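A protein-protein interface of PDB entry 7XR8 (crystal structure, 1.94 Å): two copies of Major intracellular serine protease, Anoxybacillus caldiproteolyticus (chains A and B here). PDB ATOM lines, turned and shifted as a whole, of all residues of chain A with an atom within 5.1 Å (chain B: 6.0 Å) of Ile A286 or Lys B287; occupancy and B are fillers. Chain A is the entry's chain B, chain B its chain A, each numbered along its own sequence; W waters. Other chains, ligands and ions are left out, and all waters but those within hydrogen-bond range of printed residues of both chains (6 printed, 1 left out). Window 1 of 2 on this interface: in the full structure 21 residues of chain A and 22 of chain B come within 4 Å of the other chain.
Of the 12 printed residues of chain B, 9 touch a printed residue of chain A.
Printed residues of chain B that touch a printed residue of chain A: Tyr B282, Ala B283, Gln B284, Ile B286, Lys B287, Thr B289, Ala B308, Pro B309 and Leu B312.
Hydrophobic or aromatic side chains of chain B that line the printed part of chain A: Tyr B282, Ala B283, Ile B286, Ala B308, Pro B309 and Leu B312.
Among the printed residues, no Asp or Glu carboxylate lies within 4 Å of a Lys or Arg side-chain nitrogen of the other chain.
NE2 of Gln B284 sits at hydrogen-bond distance from OD1 of Asn A301 (2.7 Å).
The side-chain amino group (NZ) of Lys B287 lies within hydrogen-bond range of the side-chain hydroxyl (OG1) of Thr A289.
O of Asn A301 is in hydrogen-bond range of NZ of Lys B287 (3.0 Å).
The side-chain amino group of Lys A287 sits at hydrogen-bond distance from the side-chain hydroxyl of Thr B289 (2.7 Å).
Tyr A282 touches Ala B283 (CE2 to CB, 3.5 Å).
Ala A283 touches Tyr B282.
Ala A283 touches Ala B283.
Ile B286 touches Ala A283 (CG2 to O, 3.7 Å).
Ala B283 touches Ile A286.
O of Ile A286 touches CE of Lys B287 (3.4 Å).
Ile B286 touches Lys A287.
CD1 of Leu B312 touches O of Thr A289, at 3.8 Å.
O of Pro B309 touches CG of Pro A291 (3.5 Å).
Leu A312 touches Ala B308 (CD2 to O, 3.6 Å).
Ala B283 touches its own counterpart, Ala A283.
Ala A283 touches Ile B286, and with the chains exchanged Ile A286 touches Ala B283.
Ile A286 touches Lys B287, and with the chains exchanged Lys A287 touches Ile B286.
Thr A289 touches Leu B312, and with the chains exchanged Leu A312 touches Thr B289.
Positions printed for both chains: 282, 283, 284, 285, 286, 287, 288, 289 and 312.
Of the 16 pairs that touch across the chains among the printed residues, 12 have their exchanged pair printed and touching as well.
Of chain B, only Ala B283 and Lys B287 come within 4 Å of Ile A286.
Printed residues of chain B within 4 Å of Leu A312: Thr B289, Ala B308 and Leu B312.
Of the printed residues of chain B, Thr A289 touches Lys B287 (2.8 Å) and Leu B312 (3.8 Å).
Printed residues of chain A within 4 Å of Ile B286: Ala A283 (3.7 Å) and Lys A287 (3.9 Å).
Printed residues of chain B within 4 Å of Asn A301: Gln B284 and Lys B287.
Printed residues of chain B within 4 Å of Lys A287: Ile B286 and Thr B289.
Val A228 touches none of the printed residues of chain B.
Water W3 bridges the side-chain amino group (NZ) of Lys B287 and the backbone carbonyl oxygen (O) of Thr A289.
Water W2 lies within hydrogen-bond range of OE1 of Gln B284 (2.7 Å), NH2 of Arg B288 (3.3 Å) and OD1 of Asn A301 (3.4 Å).
Water W4 lies within hydrogen-bond range of the side-chain amino group (NZ) of Lys A287 (2.7 Å) and the backbone carbonyl oxygen (O) of Thr B289 (2.9 Å).
Water W1 lies within hydrogen-bond range of the side-chain hydroxyl (OH) of Tyr A282 (2.8 Å), the side-chain amide nitrogen (NE2) of Gln B284 (2.9 Å) and the side-chain amide nitrogen (ND2) of Asn A301 (3.1 Å).
Water W6 bridges OH of Tyr B282 (2.8 Å) and NE2 of Gln A284 (3.2 Å).
Water W5 bridges the side-chain amino group (NZ) of Lys B287 and the backbone carbonyl oxygen (O) of Asn A301.
The side-chain amide oxygen (OE1) of Gln B284 sits at hydrogen-bond distance from the guanidinium group (NH1) of Arg B288 (2.8 Å).
O of Ile B286 lies within hydrogen-bond range of OG1 of Thr B289 (2.7 Å).
OD1 of Asp A227 lies within hydrogen-bond range of OH of Tyr A282 (2.6 Å).
O of Asp A227 is in hydrogen-bond range of N of Asn A301 (2.9 Å).
OG1 of Thr A289 is in hydrogen-bond range of O of Ile A286 (2.8 Å).
The backbone carbonyl oxygen of Asn A301 is in hydrogen-bond range of the side-chain hydroxyl of Thr A289 (3.2 Å).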
ATOM      1  N   ASP A 227     -23.176  11.775  -3.186  1.00  0.00           N
ATOM      2  CA  ASP A 227     -22.825  13.189  -3.308  1.00  0.00           C
ATOM      3  C   ASP A 227     -23.960  14.099  -2.855  1.00  0.00           C
ATOM      4  O   ASP A 227     -23.724  15.062  -2.127  1.00  0.00           O
ATOM      5  CB  ASP A 227     -22.438  13.537  -4.752  1.00  0.00           C
ATOM      6  CG  ASP A 227     -21.039  13.063  -5.107  1.00  0.00           C
ATOM      7  OD1 ASP A 227     -20.060  13.598  -4.541  1.00  0.00           O
ATOM      8  OD2 ASP A 227     -20.929  12.139  -5.933  1.00  0.00           O
ATOM      9  N   VAL A 228     -25.182  13.837  -3.323  1.00  0.00           N
ATOM     10  CA  VAL A 228     -26.358  14.668  -3.060  1.00  0.00           C
ATOM     11  C   VAL A 228     -27.566  13.741  -3.001  1.00  0.00           C
ATOM     12  O   VAL A 228     -27.513  12.600  -3.454  1.00  0.00           O
ATOM     13  CB  VAL A 228     -26.611  15.748  -4.148  1.00  0.00           C
ATOM     14  CG1 VAL A 228     -25.412  16.725  -4.298  1.00  0.00           C
ATOM     15  CG2 VAL A 228     -26.956  15.079  -5.488  1.00  0.00           C
ATOM     16  N   TYR A 282     -19.287  20.912 -10.588  1.00  0.00           N
ATOM     17  CA  TYR A 282     -19.611  20.059  -9.444  1.00  0.00           C
ATOM     18  C   TYR A 282     -19.681  20.876  -8.160  1.00  0.00           C
ATOM     19  O   TYR A 282     -20.594  20.694  -7.340  1.00  0.00           O
ATOM     20  CB  TYR A 282     -18.572  18.939  -9.307  1.00  0.00           C
ATOM     21  CG  TYR A 282     -18.705  18.157  -8.028  1.00  0.00           C
ATOM     22  CD1 TYR A 282     -19.788  17.307  -7.821  1.00  0.00           C
ATOM     23  CD2 TYR A 282     -17.746  18.259  -7.027  1.00  0.00           C
ATOM     24  CE1 TYR A 282     -19.912  16.581  -6.635  1.00  0.00           C
ATOM     25  CE2 TYR A 282     -17.874  17.552  -5.840  1.00  0.00           C
ATOM     26  CZ  TYR A 282     -18.942  16.712  -5.656  1.00  0.00           C
ATOM     27  OH  TYR A 282     -19.037  16.002  -4.477  1.00  0.00           O
ATOM     28  N   ALA A 283     -18.735  21.804  -7.982  1.00  0.00           N
ATOM     29  CA  ALA A 283     -18.771  22.677  -6.815  1.00  0.00           C
ATOM     30  C   ALA A 283     -19.988  23.592  -6.844  1.00  0.00           C
ATOM     31  O   ALA A 283     -20.535  23.931  -5.786  1.00  0.00           O
ATOM     32  CB  ALA A 283     -17.479  23.508  -6.724  1.00  0.00           C
ATOM     33  N   GLN A 284     -20.411  24.030  -8.035  1.00  0.00           N
ATOM     34  CA  GLN A 284     -21.630  24.836  -8.111  1.00  0.00           C
ATOM     35  C   GLN A 284     -22.851  24.018  -7.682  1.00  0.00           C
ATOM     36  O   GLN A 284     -23.787  24.559  -7.083  1.00  0.00           O
ATOM     37  CB  GLN A 284     -21.820  25.395  -9.527  1.00  0.00           C
ATOM     38  CG  GLN A 284     -20.746  26.398  -9.968  1.00  0.00           C
ATOM     39  CD  GLN A 284     -20.596  27.537  -8.974  1.00  0.00           C
ATOM     40  OE1 GLN A 284     -21.585  28.119  -8.528  1.00  0.00           O
ATOM     41  NE2 GLN A 284     -19.359  27.840  -8.601  1.00  0.00           N
ATOM     42  N   LEU A 285     -22.847  22.717  -7.957  1.00  0.00           N
ATOM     43  CA  LEU A 285     -23.903  21.852  -7.424  1.00  0.00           C
ATOM     44  C   LEU A 285     -23.829  21.767  -5.902  1.00  0.00           C
ATOM     45  O   LEU A 285     -24.845  21.891  -5.212  1.00  0.00           O
ATOM     46  CB  LEU A 285     -23.814  20.453  -8.030  1.00  0.00           C
ATOM     47  CG  LEU A 285     -24.808  19.430  -7.451  1.00  0.00           C
ATOM     48  CD1 LEU A 285     -26.262  19.859  -7.732  1.00  0.00           C
ATOM     49  CD2 LEU A 285     -24.572  18.060  -8.034  1.00  0.00           C
ATOM     50  N   ILE A 286     -22.636  21.508  -5.361  1.00  0.00           N
ATOM     51  CA  ILE A 286     -22.513  21.293  -3.919  1.00  0.00           C
ATOM     52  C   ILE A 286     -22.810  22.588  -3.158  1.00  0.00           C
ATOM     53  O   ILE A 286     -23.313  22.570  -2.026  1.00  0.00           O
ATOM     54  CB  ILE A 286     -21.109  20.736  -3.623  1.00  0.00           C
ATOM     55  CG1 ILE A 286     -20.891  19.396  -4.355  1.00  0.00           C
ATOM     56  CG2 ILE A 286     -20.893  20.541  -2.126  1.00  0.00           C
ATOM     57  CD1 ILE A 286     -22.048  18.392  -4.210  1.00  0.00           C
ATOM     58  N   LYS A 287     -22.533  23.728  -3.782  1.00  0.00           N
ATOM     59  CA  LYS A 287     -22.940  25.008  -3.220  1.00  0.00           C
ATOM     60  C   LYS A 287     -24.457  25.094  -3.090  1.00  0.00           C
ATOM     61  O   LYS A 287     -24.974  25.745  -2.170  1.00  0.00           O
ATOM     62  CB  LYS A 287     -22.388  26.127  -4.124  1.00  0.00           C
ATOM     63  CG  LYS A 287     -22.917  27.508  -3.891  1.00  0.00           C
ATOM     64  CD  LYS A 287     -22.194  28.483  -4.836  1.00  0.00           C
ATOM     65  CE  LYS A 287     -22.322  29.917  -4.378  1.00  0.00           C
ATOM     66  NZ  LYS A 287     -21.408  30.233  -3.247  1.00  0.00           N
ATOM     67  N   ARG A 288     -25.186  24.447  -3.992  1.00  0.00           N
ATOM     68  CA  ARG A 288     -26.644  24.540  -4.012  1.00  0.00           C
ATOM     69  C   ARG A 288     -27.271  23.278  -3.421  1.00  0.00           C
ATOM     70  O   ARG A 288     -28.081  22.586  -4.051  1.00  0.00           O
ATOM     71  CB  ARG A 288     -27.131  24.807  -5.439  1.00  0.00           C
ATOM     72  CG  ARG A 288     -26.708  26.207  -5.917  1.00  0.00           C
ATOM     73  CD  ARG A 288     -26.884  26.445  -7.398  1.00  0.00           C
ATOM     74  NE  ARG A 288     -26.503  27.817  -7.728  1.00  0.00           N
ATOM     75  CZ  ARG A 288     -25.244  28.232  -7.893  1.00  0.00           C
ATOM     76  NH1 ARG A 288     -24.233  27.373  -7.788  1.00  0.00           N
ATOM     77  NH2 ARG A 288     -24.989  29.513  -8.162  1.00  0.00           N
ATOM     78  N   THR A 289     -26.894  22.997  -2.174  1.00  0.00           N
ATOM     79  CA  THR A 289     -27.476  21.906  -1.404  1.00  0.00           C
ATOM     80  C   THR A 289     -27.928  22.403  -0.042  1.00  0.00           C
ATOM     81  O   THR A 289     -27.335  23.318   0.542  1.00  0.00           O
ATOM     82  CB  THR A 289     -26.500  20.760  -1.177  1.00  0.00           C
ATOM     83  OG1 THR A 289     -25.299  21.278  -0.593  1.00  0.00           O
ATOM     84  CG2 THR A 289     -26.202  20.026  -2.473  1.00  0.00           C
ATOM     85  N   PRO A 291     -28.414  20.957   3.713  1.00  0.00           N
ATOM     86  CA  PRO A 291     -28.251  19.835   4.645  1.00  0.00           C
ATOM     87  C   PRO A 291     -29.571  19.544   5.343  1.00  0.00           C
ATOM     88  O   PRO A 291     -30.345  20.455   5.641  1.00  0.00           O
ATOM     89  CB  PRO A 291     -27.188  20.334   5.635  1.00  0.00           C
ATOM     90  CG  PRO A 291     -26.556  21.524   4.979  1.00  0.00           C
ATOM     91  CD  PRO A 291     -27.645  22.137   4.131  1.00  0.00           C
ATOM     92  N   ASN A 301     -23.949  15.690   0.731  1.00  0.00           N
ATOM     93  CA  ASN A 301     -24.007  17.125   0.971  1.00  0.00           C
ATOM     94  C   ASN A 301     -25.416  17.643   1.175  1.00  0.00           C
ATOM     95  O   ASN A 301     -25.585  18.834   1.442  1.00  0.00           O
ATOM     96  CB  ASN A 301     -23.338  17.862  -0.195  1.00  0.00           C
ATOM     97  CG  ASN A 301     -21.867  17.575  -0.256  1.00  0.00           C
ATOM     98  OD1 ASN A 301     -21.097  18.088   0.554  1.00  0.00           O
ATOM     99  ND2 ASN A 301     -21.458  16.737  -1.205  1.00  0.00           N
ATOM    100  N   LEU A 312     -28.584  32.210   1.622  1.00  0.00           N
ATOM    101  CA  LEU A 312     -27.416  32.554   2.424  1.00  0.00           C
ATOM    102  C   LEU A 312     -27.124  34.047   2.376  1.00  0.00           C
ATOM    103  O   LEU A 312     -26.797  34.656   3.398  1.00  0.00           O
ATOM    104  CB  LEU A 312     -26.202  31.762   1.944  1.00  0.00           C
ATOM    105  CG  LEU A 312     -25.905  30.481   2.711  1.00  0.00           C
ATOM    106  CD1 LEU A 312     -24.871  29.663   1.949  1.00  0.00           C
ATOM    107  CD2 LEU A 312     -25.412  30.820   4.124  1.00  0.00           C
ATOM    108  N   TYR B 282     -12.378  20.790  -2.715  1.00  0.00           N
ATOM    109  CA  TYR B 282     -12.694  22.063  -3.359  1.00  0.00           C
ATOM    110  C   TYR B 282     -14.186  22.370  -3.264  1.00  0.00           C
ATOM    111  O   TYR B 282     -14.579  23.496  -2.939  1.00  0.00           O
ATOM    112  CB  TYR B 282     -12.255  22.047  -4.828  1.00  0.00           C
ATOM    113  CG  TYR B 282     -12.677  23.294  -5.596  1.00  0.00           C
ATOM    114  CD1 TYR B 282     -12.151  24.554  -5.277  1.00  0.00           C
ATOM    115  CD2 TYR B 282     -13.616  23.215  -6.613  1.00  0.00           C
ATOM    116  CE1 TYR B 282     -12.553  25.701  -5.970  1.00  0.00           C
ATOM    117  CE2 TYR B 282     -14.025  24.339  -7.302  1.00  0.00           C
ATOM    118  CZ  TYR B 282     -13.494  25.572  -6.988  1.00  0.00           C
ATOM    119  OH  TYR B 282     -13.920  26.675  -7.694  1.00  0.00           O
ATOM    120  N   ALA B 283     -15.038  21.374  -3.551  1.00  0.00           N
ATOM    121  CA  ALA B 283     -16.479  21.611  -3.457  1.00  0.00           C
ATOM    122  C   ALA B 283     -16.895  21.942  -2.028  1.00  0.00           C
ATOM    123  O   ALA B 283     -17.799  22.759  -1.828  1.00  0.00           O
ATOM    124  CB  ALA B 283     -17.264  20.396  -3.979  1.00  0.00           C
ATOM    125  N   GLN B 284     -16.229  21.347  -1.023  1.00  0.00           N
ATOM    126  CA  GLN B 284     -16.525  21.691   0.368  1.00  0.00           C
ATOM    127  C   GLN B 284     -16.158  23.142   0.688  1.00  0.00           C
ATOM    128  O   GLN B 284     -16.815  23.780   1.515  1.00  0.00           O
ATOM    129  CB  GLN B 284     -15.805  20.739   1.323  1.00  0.00           C
ATOM    130  CG  GLN B 284     -16.256  19.264   1.181  1.00  0.00           C
ATOM    131  CD  GLN B 284     -17.767  19.124   1.309  1.00  0.00           C
ATOM    132  OE1 GLN B 284     -18.388  19.725   2.195  1.00  0.00           O
ATOM    133  NE2 GLN B 284     -18.367  18.365   0.405  1.00  0.00           N
ATOM    134  N   LEU B 285     -15.125  23.685   0.054  1.00  0.00           N
ATOM    135  CA  LEU B 285     -14.842  25.109   0.235  1.00  0.00           C
ATOM    136  C   LEU B 285     -15.922  25.957  -0.419  1.00  0.00           C
ATOM    137  O   LEU B 285     -16.393  26.945   0.165  1.00  0.00           O
ATOM    138  CB  LEU B 285     -13.466  25.456  -0.348  1.00  0.00           C
ATOM    139  CG  LEU B 285     -13.115  26.942  -0.497  1.00  0.00           C
ATOM    140  CD1 LEU B 285     -12.968  27.653   0.873  1.00  0.00           C
ATOM    141  CD2 LEU B 285     -11.846  27.103  -1.341  1.00  0.00           C
ATOM    142  N   ILE B 286     -16.342  25.574  -1.624  1.00  0.00           N
ATOM    143  CA  ILE B 286     -17.328  26.384  -2.337  1.00  0.00           C
ATOM    144  C   ILE B 286     -18.682  26.321  -1.636  1.00  0.00           C
ATOM    145  O   ILE B 286     -19.441  27.300  -1.642  1.00  0.00           O
ATOM    146  CB  ILE B 286     -17.404  25.943  -3.810  1.00  0.00           C
ATOM    147  CG1 ILE B 286     -16.038  26.144  -4.479  1.00  0.00           C
ATOM    148  CG2 ILE B 286     -18.484  26.738  -4.581  1.00  0.00           C
ATOM    149  CD1 ILE B 286     -15.392  27.488  -4.146  1.00  0.00           C
ATOM    150  N   LYS B 287     -19.006  25.180  -1.022  1.00  0.00           N
ATOM    151  CA  LYS B 287     -20.185  25.107  -0.155  1.00  0.00           C
ATOM    152  C   LYS B 287     -20.109  26.154   0.945  1.00  0.00           C
ATOM    153  O   LYS B 287     -21.127  26.727   1.348  1.00  0.00           O
ATOM    154  CB  LYS B 287     -20.290  23.697   0.454  1.00  0.00           C
ATOM    155  CG  LYS B 287     -21.414  23.485   1.458  1.00  0.00           C
ATOM    156  CD  LYS B 287     -21.527  21.984   1.834  1.00  0.00           C
ATOM    157  CE  LYS B 287     -22.673  21.320   1.070  1.00  0.00           C
ATOM    158  NZ  LYS B 287     -23.964  21.359   1.838  1.00  0.00           N
ATOM    159  N   ARG B 288     -18.905  26.429   1.424  1.00  0.00           N
ATOM    160  CA  ARG B 288     -18.707  27.318   2.570  1.00  0.00           C
ATOM    161  C   ARG B 288     -18.299  28.715   2.100  1.00  0.00           C
ATOM    162  O   ARG B 288     -17.254  29.247   2.466  1.00  0.00           O
ATOM    163  CB  ARG B 288     -17.684  26.706   3.526  1.00  0.00           C
ATOM    164  CG  ARG B 288     -18.289  25.612   4.408  1.00  0.00           C
ATOM    165  CD  ARG B 288     -17.271  24.569   4.883  1.00  0.00           C
ATOM    166  NE  ARG B 288     -17.956  23.455   5.547  1.00  0.00           N
ATOM    167  CZ  ARG B 288     -18.340  22.340   4.932  1.00  0.00           C
ATOM    168  NH1 ARG B 288     -18.094  22.168   3.624  1.00  0.00           N
ATOM    169  NH2 ARG B 288     -18.972  21.393   5.615  1.00  0.00           N
ATOM    170  N   THR B 289     -19.164  29.307   1.265  1.00  0.00           N
ATOM    171  CA  THR B 289     -19.019  30.688   0.824  1.00  0.00           C
ATOM    172  C   THR B 289     -20.318  31.469   1.010  1.00  0.00           C
ATOM    173  O   THR B 289     -21.423  30.910   0.965  1.00  0.00           O
ATOM    174  CB  THR B 289     -18.569  30.788  -0.644  1.00  0.00           C
ATOM    175  OG1 THR B 289     -19.429  29.993  -1.486  1.00  0.00           O
ATOM    176  CG2 THR B 289     -17.124  30.335  -0.757  1.00  0.00           C
ATOM    177  N   TYR B 305     -16.848  31.452   4.236  1.00  0.00           N
ATOM    178  CA  TYR B 305     -17.809  31.660   5.321  1.00  0.00           C
ATOM    179  C   TYR B 305     -18.158  30.268   5.854  1.00  0.00           C
ATOM    180  O   TYR B 305     -19.023  29.571   5.313  1.00  0.00           O
ATOM    181  CB  TYR B 305     -19.034  32.429   4.843  1.00  0.00           C
ATOM    182  CG  TYR B 305     -19.816  33.100   5.962  1.00  0.00           C
ATOM    183  CD1 TYR B 305     -20.847  32.426   6.608  1.00  0.00           C
ATOM    184  CD2 TYR B 305     -19.520  34.397   6.371  1.00  0.00           C
ATOM    185  CE1 TYR B 305     -21.558  33.014   7.637  1.00  0.00           C
ATOM    186  CE2 TYR B 305     -20.248  35.012   7.405  1.00  0.00           C
ATOM    187  CZ  TYR B 305     -21.270  34.302   8.023  1.00  0.00           C
ATOM    188  OH  TYR B 305     -22.009  34.862   9.040  1.00  0.00           O
ATOM    189  N   ALA B 308     -21.587  28.402   6.551  1.00  0.00           N
ATOM    190  CA  ALA B 308     -22.689  28.566   5.598  1.00  0.00           C
ATOM    191  C   ALA B 308     -23.658  27.385   5.554  1.00  0.00           C
ATOM    192  O   ALA B 308     -24.874  27.626   5.618  1.00  0.00           O
ATOM    193  CB  ALA B 308     -22.137  28.881   4.199  1.00  0.00           C
ATOM    194  N   PRO B 309     -23.224  26.115   5.483  1.00  0.00           N
ATOM    195  CA  PRO B 309     -24.232  25.034   5.466  1.00  0.00           C
ATOM    196  C   PRO B 309     -25.008  24.915   6.771  1.00  0.00           C
ATOM    197  O   PRO B 309     -26.180  24.521   6.738  1.00  0.00           O
ATOM    198  CB  PRO B 309     -23.411  23.767   5.176  1.00  0.00           C
ATOM    199  CG  PRO B 309     -22.014  24.092   5.633  1.00  0.00           C
ATOM    200  CD  PRO B 309     -21.849  25.583   5.365  1.00  0.00           C
ATOM    201  N   LEU B 312     -27.898  27.304   6.488  1.00  0.00           N
ATOM    202  CA  LEU B 312     -28.953  26.812   5.608  1.00  0.00           C
ATOM    203  C   LEU B 312     -29.819  25.790   6.321  1.00  0.00           C
ATOM    204  O   LEU B 312     -31.050  25.852   6.261  1.00  0.00           O
ATOM    205  CB  LEU B 312     -28.343  26.207   4.342  1.00  0.00           C
ATOM    206  CG  LEU B 312     -27.943  27.235   3.296  1.00  0.00           C
ATOM    207  CD1 LEU B 312     -26.974  26.650   2.276  1.00  0.00           C
ATOM    208  CD2 LEU B 312     -29.212  27.764   2.636  1.00  0.00           C
HETATM  209  O   HOH W   1     -18.428  16.501  -1.837  1.00  0.00           O
HETATM  210  O   HOH W   2     -20.446  19.118   3.764  1.00  0.00           O
HETATM  211  O   HOH W   3     -24.857  23.759   1.980  1.00  0.00           O
HETATM  212  O   HOH W   4     -23.129  29.977  -1.173  1.00  0.00           O
HETATM  213  O   HOH W   5     -23.461  19.612   4.073  1.00  0.00           O
HETATM  214  O   HOH W   6     -16.209  27.618  -9.091  1.00  0.00           O
